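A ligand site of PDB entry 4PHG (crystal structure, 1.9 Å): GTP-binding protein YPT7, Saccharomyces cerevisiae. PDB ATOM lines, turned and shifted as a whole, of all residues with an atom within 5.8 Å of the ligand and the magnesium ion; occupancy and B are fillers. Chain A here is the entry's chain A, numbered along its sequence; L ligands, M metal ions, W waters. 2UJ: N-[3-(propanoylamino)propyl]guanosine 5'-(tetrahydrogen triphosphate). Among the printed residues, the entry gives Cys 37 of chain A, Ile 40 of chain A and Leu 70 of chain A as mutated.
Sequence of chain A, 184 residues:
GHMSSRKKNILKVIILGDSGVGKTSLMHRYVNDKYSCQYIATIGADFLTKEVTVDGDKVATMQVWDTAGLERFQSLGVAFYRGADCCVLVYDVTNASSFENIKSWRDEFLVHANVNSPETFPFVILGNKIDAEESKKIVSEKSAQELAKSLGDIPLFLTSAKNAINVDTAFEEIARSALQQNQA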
ATOM      1  N   GLY A  17     -24.049   6.496  32.146  1.00  0.00           N
ATOM      2  CA  GLY A  17     -24.937   6.301  31.066  1.00  0.00           C
ATOM      3  C   GLY A  17     -25.390   4.841  30.988  1.00  0.00           C
ATOM      4  O   GLY A  17     -24.818   3.939  31.594  1.00  0.00           O
ATOM      5  N   ASP A  18     -26.424   4.595  30.254  1.00  0.00           N
ATOM      6  CA  ASP A  18     -27.027   3.243  30.250  1.00  0.00           C
ATOM      7  C   ASP A  18     -26.042   2.176  29.719  1.00  0.00           C
ATOM      8  O   ASP A  18     -25.085   2.511  28.935  1.00  0.00           O
ATOM      9  CB  ASP A  18     -28.316   3.212  29.421  1.00  0.00           C
ATOM     10  CG  ASP A  18     -29.455   3.992  30.058  1.00  0.00           C
ATOM     11  OD1 ASP A  18     -29.292   4.478  31.175  1.00  0.00           O
ATOM     12  OD2 ASP A  18     -30.520   4.134  29.404  1.00  0.00           O
ATOM     13  N   SER A  19     -26.275   0.933  30.133  1.00  0.00           N
ATOM     14  CA  SER A  19     -25.577  -0.228  29.527  1.00  0.00           C
ATOM     15  C   SER A  19     -25.620  -0.243  27.993  1.00  0.00           C
ATOM     16  O   SER A  19     -26.690  -0.117  27.355  1.00  0.00           O
ATOM     17  CB  SER A  19     -26.166  -1.557  30.029  1.00  0.00           C
ATOM     18  OG  SER A  19     -25.872  -1.679  31.402  1.00  0.00           O
ATOM     19  N   GLY A  20     -24.457  -0.398  27.379  1.00  0.00           N
ATOM     20  CA  GLY A  20     -24.365  -0.539  25.926  1.00  0.00           C
ATOM     21  C   GLY A  20     -24.107   0.748  25.127  1.00  0.00           C
ATOM     22  O   GLY A  20     -23.928   0.672  23.891  1.00  0.00           O
ATOM     23  N   VAL A  21     -24.137   1.921  25.778  1.00  0.00           N
ATOM     24  CA  VAL A  21     -24.054   3.176  25.019  1.00  0.00           C
ATOM     25  C   VAL A  21     -22.647   3.468  24.433  1.00  0.00           C
ATOM     26  O   VAL A  21     -22.527   4.298  23.543  1.00  0.00           O
ATOM     27  CB  VAL A  21     -24.556   4.428  25.826  1.00  0.00           C
ATOM     28  CG1 VAL A  21     -26.038   4.349  26.196  1.00  0.00           C
ATOM     29  CG2 VAL A  21     -23.674   4.720  27.055  1.00  0.00           C
ATOM     30  N   GLY A  22     -21.620   2.882  25.034  1.00  0.00           N
ATOM     31  CA  GLY A  22     -20.224   3.041  24.621  1.00  0.00           C
ATOM     32  C   GLY A  22     -19.308   3.691  25.583  1.00  0.00           C
ATOM     33  O   GLY A  22     -18.268   4.231  25.152  1.00  0.00           O
ATOM     34  N   LYS A  23     -19.625   3.663  26.885  1.00  0.00           N
ATOM     35  CA  LYS A  23     -18.778   4.307  27.888  1.00  0.00           C
ATOM     36  C   LYS A  23     -17.342   3.755  27.928  1.00  0.00           C
ATOM     37  O   LYS A  23     -16.318   4.519  27.905  1.00  0.00           O
ATOM     38  CB  LYS A  23     -19.400   4.181  29.272  1.00  0.00           C
ATOM     39  CG  LYS A  23     -20.838   4.739  29.431  1.00  0.00           C
ATOM     40  CD  LYS A  23     -21.357   4.556  30.847  1.00  0.00           C
ATOM     41  CE  LYS A  23     -21.515   3.149  31.284  1.00  0.00           C
ATOM     42  NZ  LYS A  23     -22.538   2.405  30.421  1.00  0.00           N
ATOM     43  N   THR A  24     -17.238   2.430  28.024  1.00  0.00           N
ATOM     44  CA  THR A  24     -15.901   1.761  28.060  1.00  0.00           C
ATOM     45  C   THR A  24     -15.176   1.979  26.714  1.00  0.00           C
ATOM     46  O   THR A  24     -13.968   2.236  26.708  1.00  0.00           O
ATOM     47  CB  THR A  24     -16.075   0.277  28.352  1.00  0.00           C
ATOM     48  OG1 THR A  24     -16.674   0.147  29.651  1.00  0.00           O
ATOM     49  CG2 THR A  24     -14.729  -0.503  28.305  1.00  0.00           C
ATOM     50  N   SER A  25     -15.938   1.934  25.601  1.00  0.00           N
ATOM     51  CA  SER A  25     -15.350   2.158  24.292  1.00  0.00           C
ATOM     52  C   SER A  25     -14.795   3.585  24.177  1.00  0.00           C
ATOM     53  O   SER A  25     -13.690   3.772  23.679  1.00  0.00           O
ATOM     54  CB  SER A  25     -16.315   1.787  23.171  1.00  0.00           C
ATOM     55  OG  SER A  25     -16.744   0.423  23.260  1.00  0.00           O
ATOM     56  N   LEU A  26     -15.506   4.604  24.721  1.00  0.00           N
ATOM     57  CA  LEU A  26     -15.029   5.960  24.583  1.00  0.00           C
ATOM     58  C   LEU A  26     -13.786   6.150  25.437  1.00  0.00           C
ATOM     59  O   LEU A  26     -12.800   6.796  24.999  1.00  0.00           O
ATOM     60  CB  LEU A  26     -16.159   6.948  24.940  1.00  0.00           C
ATOM     61  CG  LEU A  26     -17.329   7.118  24.010  1.00  0.00           C
ATOM     62  CD1 LEU A  26     -18.532   7.798  24.684  1.00  0.00           C
ATOM     63  CD2 LEU A  26     -16.935   7.898  22.754  1.00  0.00           C
ATOM     64  N   TYR A  35     -10.345   0.010  20.161  1.00  0.00           N
ATOM     65  CA  TYR A  35     -11.778  -0.155  19.981  1.00  0.00           C
ATOM     66  C   TYR A  35     -11.960  -1.631  19.563  1.00  0.00           C
ATOM     67  O   TYR A  35     -11.163  -2.139  18.809  1.00  0.00           O
ATOM     68  CB  TYR A  35     -12.363   0.773  18.882  1.00  0.00           C
ATOM     69  CG  TYR A  35     -13.775   0.380  18.511  1.00  0.00           C
ATOM     70  CD1 TYR A  35     -14.859   0.667  19.367  1.00  0.00           C
ATOM     71  CD2 TYR A  35     -14.032  -0.326  17.355  1.00  0.00           C
ATOM     72  CE1 TYR A  35     -16.164   0.279  19.056  1.00  0.00           C
ATOM     73  CE2 TYR A  35     -15.293  -0.768  17.037  1.00  0.00           C
ATOM     74  CZ  TYR A  35     -16.373  -0.451  17.879  1.00  0.00           C
ATOM     75  OH  TYR A  35     -17.634  -0.905  17.529  1.00  0.00           O
ATOM     76  N   SER A  36     -12.993  -2.294  20.071  1.00  0.00           N
ATOM     77  CA  SER A  36     -13.429  -3.599  19.637  1.00  0.00           C
ATOM     78  C   SER A  36     -14.931  -3.537  19.376  1.00  0.00           C
ATOM     79  O   SER A  36     -15.673  -2.854  20.111  1.00  0.00           O
ATOM     80  CB  SER A  36     -13.139  -4.643  20.723  1.00  0.00           C
ATOM     81  OG  SER A  36     -13.795  -5.879  20.431  1.00  0.00           O
ATOM     82  N   CYS A  37     -15.337  -4.168  18.267  1.00  0.00           N
ATOM     83  CA  CYS A  37     -16.726  -4.403  17.904  1.00  0.00           C
ATOM     84  C   CYS A  37     -17.489  -5.267  18.897  1.00  0.00           C
ATOM     85  O   CYS A  37     -18.691  -5.209  18.955  1.00  0.00           O
ATOM     86  CB  CYS A  37     -16.770  -5.197  16.583  1.00  0.00           C
ATOM     87  SG  CYS A  37     -16.131  -4.282  15.148  1.00  0.00           S
ATOM     88  N   GLN A  38     -16.753  -6.129  19.582  1.00  0.00           N
ATOM     89  CA  GLN A  38     -17.244  -7.020  20.583  1.00  0.00           C
ATOM     90  C   GLN A  38     -17.646  -6.239  21.822  1.00  0.00           C
ATOM     91  O   GLN A  38     -17.004  -5.252  22.170  1.00  0.00           O
ATOM     92  CB  GLN A  38     -16.106  -8.009  20.997  1.00  0.00           C
ATOM     93  CG  GLN A  38     -16.092  -9.351  20.268  1.00  0.00           C
ATOM     94  CD  GLN A  38     -16.460  -9.258  18.806  1.00  0.00           C
ATOM     95  OE1 GLN A  38     -15.756  -8.628  17.980  1.00  0.00           O
ATOM     96  NE2 GLN A  38     -17.579  -9.898  18.453  1.00  0.00           N
ATOM     97  N   TYR A  39     -18.693  -6.719  22.475  1.00  0.00           N
ATOM     98  CA  TYR A  39     -19.218  -6.108  23.667  1.00  0.00           C
ATOM     99  C   TYR A  39     -18.809  -6.964  24.825  1.00  0.00           C
ATOM    100  O   TYR A  39     -19.128  -8.145  24.845  1.00  0.00           O
ATOM    101  CB  TYR A  39     -20.732  -6.023  23.580  1.00  0.00           C
ATOM    102  CG  TYR A  39     -21.461  -5.467  24.813  1.00  0.00           C
ATOM    103  CD1 TYR A  39     -20.865  -4.541  25.689  1.00  0.00           C
ATOM    104  CD2 TYR A  39     -22.771  -5.848  25.067  1.00  0.00           C
ATOM    105  CE1 TYR A  39     -21.543  -4.025  26.793  1.00  0.00           C
ATOM    106  CE2 TYR A  39     -23.448  -5.346  26.169  1.00  0.00           C
ATOM    107  CZ  TYR A  39     -22.847  -4.445  27.025  1.00  0.00           C
ATOM    108  OH  TYR A  39     -23.567  -3.998  28.146  1.00  0.00           O
ATOM    109  N   ILE A  40     -18.102  -6.377  25.784  1.00  0.00           N
ATOM    110  CA  ILE A  40     -17.857  -6.992  27.097  1.00  0.00           C
ATOM    111  C   ILE A  40     -18.366  -6.019  28.174  1.00  0.00           C
ATOM    112  O   ILE A  40     -17.783  -4.916  28.358  1.00  0.00           O
ATOM    113  CB  ILE A  40     -16.346  -7.383  27.314  1.00  0.00           C
ATOM    114  CG1 ILE A  40     -15.891  -8.286  26.165  1.00  0.00           C
ATOM    115  CG2 ILE A  40     -16.106  -8.041  28.692  1.00  0.00           C
ATOM    116  CD1 ILE A  40     -14.419  -8.629  26.258  1.00  0.00           C
ATOM    117  N   ALA A  41     -19.487  -6.415  28.817  1.00  0.00           N
ATOM    118  CA  ALA A  41     -20.108  -5.615  29.875  1.00  0.00           C
ATOM    119  C   ALA A  41     -19.105  -5.383  30.984  1.00  0.00           C
ATOM    120  O   ALA A  41     -18.324  -6.258  31.354  1.00  0.00           O
ATOM    121  CB  ALA A  41     -21.394  -6.269  30.426  1.00  0.00           C
ATOM    122  N   THR A  42     -19.140  -4.179  31.540  1.00  0.00           N
ATOM    123  CA  THR A  42     -18.164  -3.806  32.521  1.00  0.00           C
ATOM    124  C   THR A  42     -18.629  -4.412  33.852  1.00  0.00           C
ATOM    125  O   THR A  42     -19.766  -4.240  34.254  1.00  0.00           O
ATOM    126  CB  THR A  42     -18.014  -2.276  32.577  1.00  0.00           C
ATOM    127  OG1 THR A  42     -17.630  -1.809  31.256  1.00  0.00           O
ATOM    128  CG2 THR A  42     -16.988  -1.847  33.643  1.00  0.00           C
ATOM    129  N   ASP A  66     -14.894   4.265  35.100  1.00  0.00           N
ATOM    130  CA  ASP A  66     -15.849   3.516  34.302  1.00  0.00           C
ATOM    131  C   ASP A  66     -16.390   2.322  35.133  1.00  0.00           C
ATOM    132  O   ASP A  66     -15.630   1.626  35.802  1.00  0.00           O
ATOM    133  CB  ASP A  66     -15.097   3.043  33.030  1.00  0.00           C
ATOM    134  CG  ASP A  66     -15.997   2.308  32.068  1.00  0.00           C
ATOM    135  OD1 ASP A  66     -17.130   2.822  31.886  1.00  0.00           O
ATOM    136  OD2 ASP A  66     -15.512   1.309  31.467  1.00  0.00           O
ATOM    137  N   THR A  67     -17.700   2.169  35.203  1.00  0.00           N
ATOM    138  CA  THR A  67     -18.313   1.028  35.794  1.00  0.00           C
ATOM    139  C   THR A  67     -19.554   0.587  34.952  1.00  0.00           C
ATOM    140  O   THR A  67     -19.773   1.044  33.850  1.00  0.00           O
ATOM    141  CB  THR A  67     -18.684   1.312  37.275  1.00  0.00           C
ATOM    142  OG1 THR A  67     -19.093   0.108  37.858  1.00  0.00           O
ATOM    143  CG2 THR A  67     -19.820   2.432  37.413  1.00  0.00           C
ATOM    144  N   ALA A  68     -20.289  -0.377  35.454  1.00  0.00           N
ATOM    145  CA  ALA A  68     -21.427  -0.870  34.735  1.00  0.00           C
ATOM    146  C   ALA A  68     -22.516   0.194  34.553  1.00  0.00           C
ATOM    147  O   ALA A  68     -22.835   0.933  35.490  1.00  0.00           O
ATOM    148  CB  ALA A  68     -21.977  -2.088  35.453  1.00  0.00           C
ATOM    149  N   GLY A  69     -23.128   0.212  33.367  1.00  0.00           N
ATOM    150  CA  GLY A  69     -24.214   1.159  33.028  1.00  0.00           C
ATOM    151  C   GLY A  69     -25.471   1.069  33.828  1.00  0.00           C
ATOM    152  O   GLY A  69     -25.926   2.054  34.363  1.00  0.00           O
ATOM    153  N   LEU A  70     -26.027  -0.126  33.959  1.00  0.00           N
ATOM    154  CA  LEU A  70     -27.276  -0.261  34.714  1.00  0.00           C
ATOM    155  C   LEU A  70     -26.959  -0.259  36.204  1.00  0.00           C
ATOM    156  O   LEU A  70     -26.006  -0.947  36.672  1.00  0.00           O
ATOM    157  CB  LEU A  70     -28.113  -1.487  34.280  1.00  0.00           C
ATOM    158  CG  LEU A  70     -27.847  -2.898  34.823  1.00  0.00           C
ATOM    159  CD1 LEU A  70     -29.184  -3.490  35.308  1.00  0.00           C
ATOM    160  CD2 LEU A  70     -27.129  -3.796  33.779  1.00  0.00           C
ATOM    161  N   ASN A 128     -23.005   9.170  21.523  1.00  0.00           N
ATOM    162  CA  ASN A 128     -22.087   8.225  20.893  1.00  0.00           C
ATOM    163  C   ASN A 128     -22.751   7.455  19.808  1.00  0.00           C
ATOM    164  O   ASN A 128     -23.967   7.287  19.781  1.00  0.00           O
ATOM    165  CB  ASN A 128     -21.576   7.242  21.954  1.00  0.00           C
ATOM    166  CG  ASN A 128     -20.424   6.419  21.460  1.00  0.00           C
ATOM    167  OD1 ASN A 128     -20.289   5.193  21.774  1.00  0.00           O
ATOM    168  ND2 ASN A 128     -19.565   7.064  20.736  1.00  0.00           N
ATOM    169  N   LYS A 129     -21.906   6.859  18.967  1.00  0.00           N
ATOM    170  CA  LYS A 129     -22.342   5.925  17.886  1.00  0.00           C
ATOM    171  C   LYS A 129     -22.782   6.698  16.686  1.00  0.00           C
ATOM    172  O   LYS A 129     -23.611   6.187  15.901  1.00  0.00           O
ATOM    173  CB  LYS A 129     -23.404   4.906  18.331  1.00  0.00           C
ATOM    174  CG  LYS A 129     -22.988   4.094  19.544  1.00  0.00           C
ATOM    175  CD  LYS A 129     -23.592   2.687  19.589  1.00  0.00           C
ATOM    176  CE  LYS A 129     -23.370   1.992  20.909  1.00  0.00           C
ATOM    177  NZ  LYS A 129     -24.126   0.729  21.147  1.00  0.00           N
ATOM    178  N   ILE A 130     -22.168   7.868  16.477  1.00  0.00           N
ATOM    179  CA  ILE A 130     -22.566   8.772  15.328  1.00  0.00           C
ATOM    180  C   ILE A 130     -22.223   8.143  13.990  1.00  0.00           C
ATOM    181  O   ILE A 130     -22.808   8.451  12.966  1.00  0.00           O
ATOM    182  CB  ILE A 130     -21.966  10.225  15.517  1.00  0.00           C
ATOM    183  CG1 ILE A 130     -22.893  11.262  14.929  1.00  0.00           C
ATOM    184  CG2 ILE A 130     -20.512  10.362  14.996  1.00  0.00           C
ATOM    185  CD1 ILE A 130     -24.368  11.125  15.307  1.00  0.00           C
ATOM    186  N   ASP A 131     -21.351   7.147  14.002  1.00  0.00           N
ATOM    187  CA  ASP A 131     -21.053   6.376  12.774  1.00  0.00           C
ATOM    188  C   ASP A 131     -22.165   5.427  12.319  1.00  0.00           C
ATOM    189  O   ASP A 131     -22.066   4.875  11.233  1.00  0.00           O
ATOM    190  CB  ASP A 131     -19.797   5.542  12.991  1.00  0.00           C
ATOM    191  CG  ASP A 131     -19.991   4.525  14.133  1.00  0.00           C
ATOM    192  OD1 ASP A 131     -19.861   4.931  15.316  1.00  0.00           O
ATOM    193  OD2 ASP A 131     -20.393   3.392  13.825  1.00  0.00           O
ATOM    194  N   ALA A 132     -23.197   5.229  13.130  1.00  0.00           N
ATOM    195  CA  ALA A 132     -24.232   4.178  12.917  1.00  0.00           C
ATOM    196  C   ALA A 132     -24.974   4.333  11.611  1.00  0.00           C
ATOM    197  O   ALA A 132     -25.153   5.442  11.127  1.00  0.00           O
ATOM    198  CB  ALA A 132     -25.271   4.187  14.040  1.00  0.00           C
ATOM    199  N   THR A 159     -20.102  11.828  19.085  1.00  0.00           N
ATOM    200  CA  THR A 159     -18.873  11.015  19.033  1.00  0.00           C
ATOM    201  C   THR A 159     -19.069   9.645  18.365  1.00  0.00           C
ATOM    202  O   THR A 159     -20.198   9.121  18.240  1.00  0.00           O
ATOM    203  CB  THR A 159     -18.328  10.780  20.482  1.00  0.00           C
ATOM    204  OG1 THR A 159     -19.295   9.990  21.202  1.00  0.00           O
ATOM    205  CG2 THR A 159     -18.190  11.997  21.164  1.00  0.00           C
ATOM    206  N   SER A 160     -17.941   9.103  17.893  1.00  0.00           N
ATOM    207  CA  SER A 160     -17.818   7.713  17.565  1.00  0.00           C
ATOM    208  C   SER A 160     -16.510   7.205  18.190  1.00  0.00           C
ATOM    209  O   SER A 160     -15.378   7.611  17.779  1.00  0.00           O
ATOM    210  CB  SER A 160     -17.806   7.536  16.033  1.00  0.00           C
ATOM    211  OG  SER A 160     -17.676   6.154  15.696  1.00  0.00           O
ATOM    212  N   ALA A 161     -16.649   6.354  19.199  1.00  0.00           N
ATOM    213  CA  ALA A 161     -15.524   5.572  19.736  1.00  0.00           C
ATOM    214  C   ALA A 161     -14.976   4.674  18.636  1.00  0.00           C
ATOM    215  O   ALA A 161     -13.779   4.519  18.487  1.00  0.00           O
ATOM    216  CB  ALA A 161     -15.953   4.738  20.887  1.00  0.00           C
ATOM    217  N   LYS A 162     -15.885   4.148  17.835  1.00  0.00           N
ATOM    218  CA  LYS A 162     -15.490   3.291  16.706  1.00  0.00           C
ATOM    219  C   LYS A 162     -14.571   3.971  15.689  1.00  0.00           C
ATOM    220  O   LYS A 162     -13.515   3.480  15.438  1.00  0.00           O
ATOM    221  CB  LYS A 162     -16.690   2.684  15.968  1.00  0.00           C
ATOM    222  CG  LYS A 162     -16.254   1.942  14.713  1.00  0.00           C
ATOM    223  CD  LYS A 162     -17.236   0.947  14.137  1.00  0.00           C
ATOM    224  CE  LYS A 162     -16.659   0.275  12.873  1.00  0.00           C
ATOM    225  NZ  LYS A 162     -16.623   1.216  11.722  1.00  0.00           N
ATOM    226  N   ASN A 163     -14.992   5.068  15.098  1.00  0.00           N
ATOM    227  CA  ASN A 163     -14.225   5.684  14.033  1.00  0.00           C
ATOM    228  C   ASN A 163     -13.379   6.873  14.483  1.00  0.00           C
ATOM    229  O   ASN A 163     -12.899   7.606  13.622  1.00  0.00           O
ATOM    230  CB  ASN A 163     -15.134   6.164  12.891  1.00  0.00           C
ATOM    231  CG  ASN A 163     -15.839   5.048  12.144  1.00  0.00           C
ATOM    232  OD1 ASN A 163     -16.841   5.300  11.485  1.00  0.00           O
ATOM    233  ND2 ASN A 163     -15.304   3.865  12.190  1.00  0.00           N
HETATM  234  OAB 2UJ L   1     -19.116  -2.171  12.521  1.00  0.00           O
HETATM  235  CBB 2UJ L   1     -19.438  -2.773  13.548  1.00  0.00           C
HETATM  236  CAN 2UJ L   1     -18.581  -3.852  14.166  1.00  0.00           C
HETATM  237  CAA 2UJ L   1     -17.246  -3.182  14.645  1.00  0.00           C
HETATM  238  NAU 2UJ L   1     -20.590  -2.532  14.152  1.00  0.00           N
HETATM  239  CAP 2UJ L   1     -21.549  -1.563  13.524  1.00  0.00           C
HETATM  240  CAO 2UJ L   1     -21.923  -0.282  14.308  1.00  0.00           C
HETATM  241  CAQ 2UJ L   1     -20.924  -0.067  15.432  1.00  0.00           C
HETATM  242  N2  2UJ L   1     -21.109   1.315  15.880  1.00  0.00           N
HETATM  243  C2  2UJ L   1     -20.581   1.730  17.043  1.00  0.00           C
HETATM  244  N3  2UJ L   1     -20.528   0.862  18.076  1.00  0.00           N
HETATM  245  N1  2UJ L   1     -20.087   3.047  17.205  1.00  0.00           N
HETATM  246  C6  2UJ L   1     -19.487   3.420  18.382  1.00  0.00           C
HETATM  247  O6  2UJ L   1     -19.094   4.592  18.470  1.00  0.00           O
HETATM  248  C5  2UJ L   1     -19.504   2.549  19.426  1.00  0.00           C
HETATM  249  C4  2UJ L   1     -20.012   1.296  19.267  1.00  0.00           C
HETATM  250  N7  2UJ L   1     -19.011   2.618  20.681  1.00  0.00           N
HETATM  251  C8  2UJ L   1     -19.259   1.468  21.277  1.00  0.00           C
HETATM  252  N9  2UJ L   1     -19.866   0.645  20.423  1.00  0.00           N
HETATM  253  C1' 2UJ L   1     -20.258  -0.742  20.549  1.00  0.00           C
HETATM  254  O4' 2UJ L   1     -21.362  -0.877  21.409  1.00  0.00           O
HETATM  255  C2' 2UJ L   1     -19.098  -1.562  21.176  1.00  0.00           C
HETATM  256  O2' 2UJ L   1     -18.271  -2.033  20.164  1.00  0.00           O
HETATM  257  C3' 2UJ L   1     -19.854  -2.685  21.875  1.00  0.00           C
HETATM  258  O3' 2UJ L   1     -20.156  -3.691  20.911  1.00  0.00           O
HETATM  259  C4' 2UJ L   1     -21.181  -2.016  22.299  1.00  0.00           C
HETATM  260  C5' 2UJ L   1     -21.201  -1.452  23.744  1.00  0.00           C
HETATM  261  O5' 2UJ L   1     -19.901  -0.779  23.986  1.00  0.00           O
HETATM  262  PA  2UJ L   1     -19.409  -0.606  25.465  1.00  0.00           P
HETATM  263  O1A 2UJ L   1     -18.288   0.474  25.451  1.00  0.00           O
HETATM  264  O2A 2UJ L   1     -19.053  -1.901  26.015  1.00  0.00           O
HETATM  265  O3A 2UJ L   1     -20.626   0.118  26.254  1.00  0.00           O
HETATM  266  PB  2UJ L   1     -20.771   0.418  27.857  1.00  0.00           P
HETATM  267  O1B 2UJ L   1     -21.578   1.674  27.898  1.00  0.00           O
HETATM  268  O2B 2UJ L   1     -19.315   0.390  28.374  1.00  0.00           O
HETATM  269  O3B 2UJ L   1     -21.648  -0.785  28.473  1.00  0.00           O
HETATM  270  PG  2UJ L   1     -21.662  -1.425  30.062  1.00  0.00           P
HETATM  271  O1G 2UJ L   1     -22.517  -2.606  29.852  1.00  0.00           O
HETATM  272  O2G 2UJ L   1     -20.270  -1.725  30.440  1.00  0.00           O
HETATM  273  O3G 2UJ L   1     -22.255  -0.336  30.766  1.00  0.00           O
HETATM  274 MG    MG M   1     -18.617  -0.680  30.009  1.00  0.00          MG
HETATM  275  O   HOH W   1     -18.171  -2.159  28.601  1.00  0.00           O
HETATM  276  O   HOH W   2     -16.487  -2.564  22.618  1.00  0.00           O
HETATM  277  O   HOH W   3     -17.178  -3.658  25.376  1.00  0.00           O
HETATM  278  O   HOH W   4     -18.855   0.947  31.375  1.00  0.00           O
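The side-chain hydroxyl (OH) of Tyr 39 is in hydrogen-bond range of an oxygen (O1G) of the ligand, at 2.4 Å. N of Thr 24 lies within hydrogen-bond range of O1A of the ligand (3.4 Å). An oxygen (O6) of the ligand sits at hydrogen-bond distance from the backbone NH (N) of Lys 162 (3.3 Å). An oxygen (O1B) of the ligand sits at hydrogen-bond distance from the backbone NH (N) of Val 21, 3.3 Å away. An oxygen (O3B) of the ligand lies within hydrogen-bond range of the backbone NH (N) of Gly 20, 3.0 Å away. An oxygen (O3G) of the ligand is in salt-bridge range of the side-chain amino group (NZ) of Lys 23, at 2.8 Å. An oxygen (O2') of the ligand is in hydrogen-bond range of the backbone carbonyl oxygen (O) of Ser 36 (2.7 Å). OD1 of Asn 128 lies close to N7 of the ligand, at 3.1 Å. O1B of the ligand sits at hydrogen-bond distance from N of Gly 22, at 3.1 Å. N of Gly 69 sits at hydrogen-bond distance from O3G of the ligand (2.8 Å). O2' of the ligand sits at hydrogen-bond distance from OH of Tyr 35, 2.9 Å away. The side-chain carboxylate (OD1) of Asp 131 lies within hydrogen-bond range of a nitrogen (N1) of the ligand (2.7 Å). The side-chain hydroxyl (OG) of Ser 25 is in hydrogen-bond range of an oxygen (O1A) of the ligand. The backbone carbonyl oxygen of Cys 37 sits at hydrogen-bond distance from an oxygen (O3') of the ligand, 2.9 Å away. NZ of Lys 129 sits at hydrogen-bond distance from O4' of the ligand. O6 of the ligand lies within hydrogen-bond range of OG of Ser 160, 3.5 Å away. The backbone NH (N) of Ala 161 sits at hydrogen-bond distance from an oxygen (O6) of the ligand (3.1 Å). The backbone NH of Thr 42 sits close to an oxygen (O2G) of the ligand (2.9 Å). The side-chain sulfur (SG) of Cys 37 is covalently linked to a carbon (CAA) of the ligand (1.6 Å). The backbone NH (N) of Ser 25 is in hydrogen-bond range of an oxygen (O1A) of the ligand, 2.8 Å away. The backbone NH of Lys 23 sits at hydrogen-bond distance from an oxygen (O1B) of the ligand (3.0 Å).
The side-chain carboxylate (OD2) of Asp 66 lies close to the side-chain hydroxyl (OG1) of Thr 24 (2.4 Å). The side-chain amide nitrogen of Asn 128 lies within hydrogen-bond range of the side-chain hydroxyl of Thr 159, at 3.0 Å. The side-chain amino group of Lys 23 sits at hydrogen-bond distance from the backbone carbonyl oxygen of Asp 18, 3.0 Å away. The backbone NH of Asn 163 sits at hydrogen-bond distance from the side-chain hydroxyl of Ser 160 (3.0 Å). The backbone NH (N) of Lys 129 lies within hydrogen-bond range of the backbone carbonyl oxygen (O) of Thr 159. The side-chain hydroxyl (OG) of Ser 160 sits close to the backbone NH (N) of Lys 162. The side-chain amino group of Lys 162 lies close to the side-chain amide nitrogen of Asn 163, at 3.0 Å. The backbone carbonyl oxygen (O) of Val 21 sits close to the side-chain amide oxygen (OD1) of Asn 128 (3.0 Å).
O of Asp 18 touches O1B of the ligand (3.8 Å). CA of Ser 19 touches O3G of the ligand, 3.5 Å away. C of Gln 38 touches O3' of the ligand, at 3.7 Å. CA of Ala 41 touches O1G of the ligand (3.9 Å). Ala 68 touches the ligand (C to O3G, 3.8 Å). Hydrophobic or aromatic side chains within 4 Å of the ligand: Val 21, Tyr 35, Tyr 39, Ala 41 and Ala 161. The nearest printed residue that does not touch the ligand is Ile 40 (4.02 Å).
Asp 66 touches the magnesium ion. Three residues have an atom within 4 Å of the magnesium ion: Thr 24, Thr 42 and Asp 66.
The magnesium ion is bound by OG1 of Thr 42 (2.0 Å), O2G of the ligand (2.0 Å), O2B of the ligand (2.1 Å), water W1 (2.1 Å), water W4 (2.1 Å) and OG1 of Thr 24 (2.1 Å).
Water W1 lies within hydrogen-bond range of O2A of the ligand (2.7 Å) and O of Ile 40 (2.8 Å). Water W4 lies within hydrogen-bond range of OD1 of Asp 66 (2.6 Å) and O of Thr 67 (2.6 Å). Water W3 bridges an oxygen (O2A) of the ligand and the backbone NH of Ile 40. Water W2 lies within hydrogen-bond range of O of Ser 36, O of Gln 38, OG of Ser 25 and O2' of the ligand.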
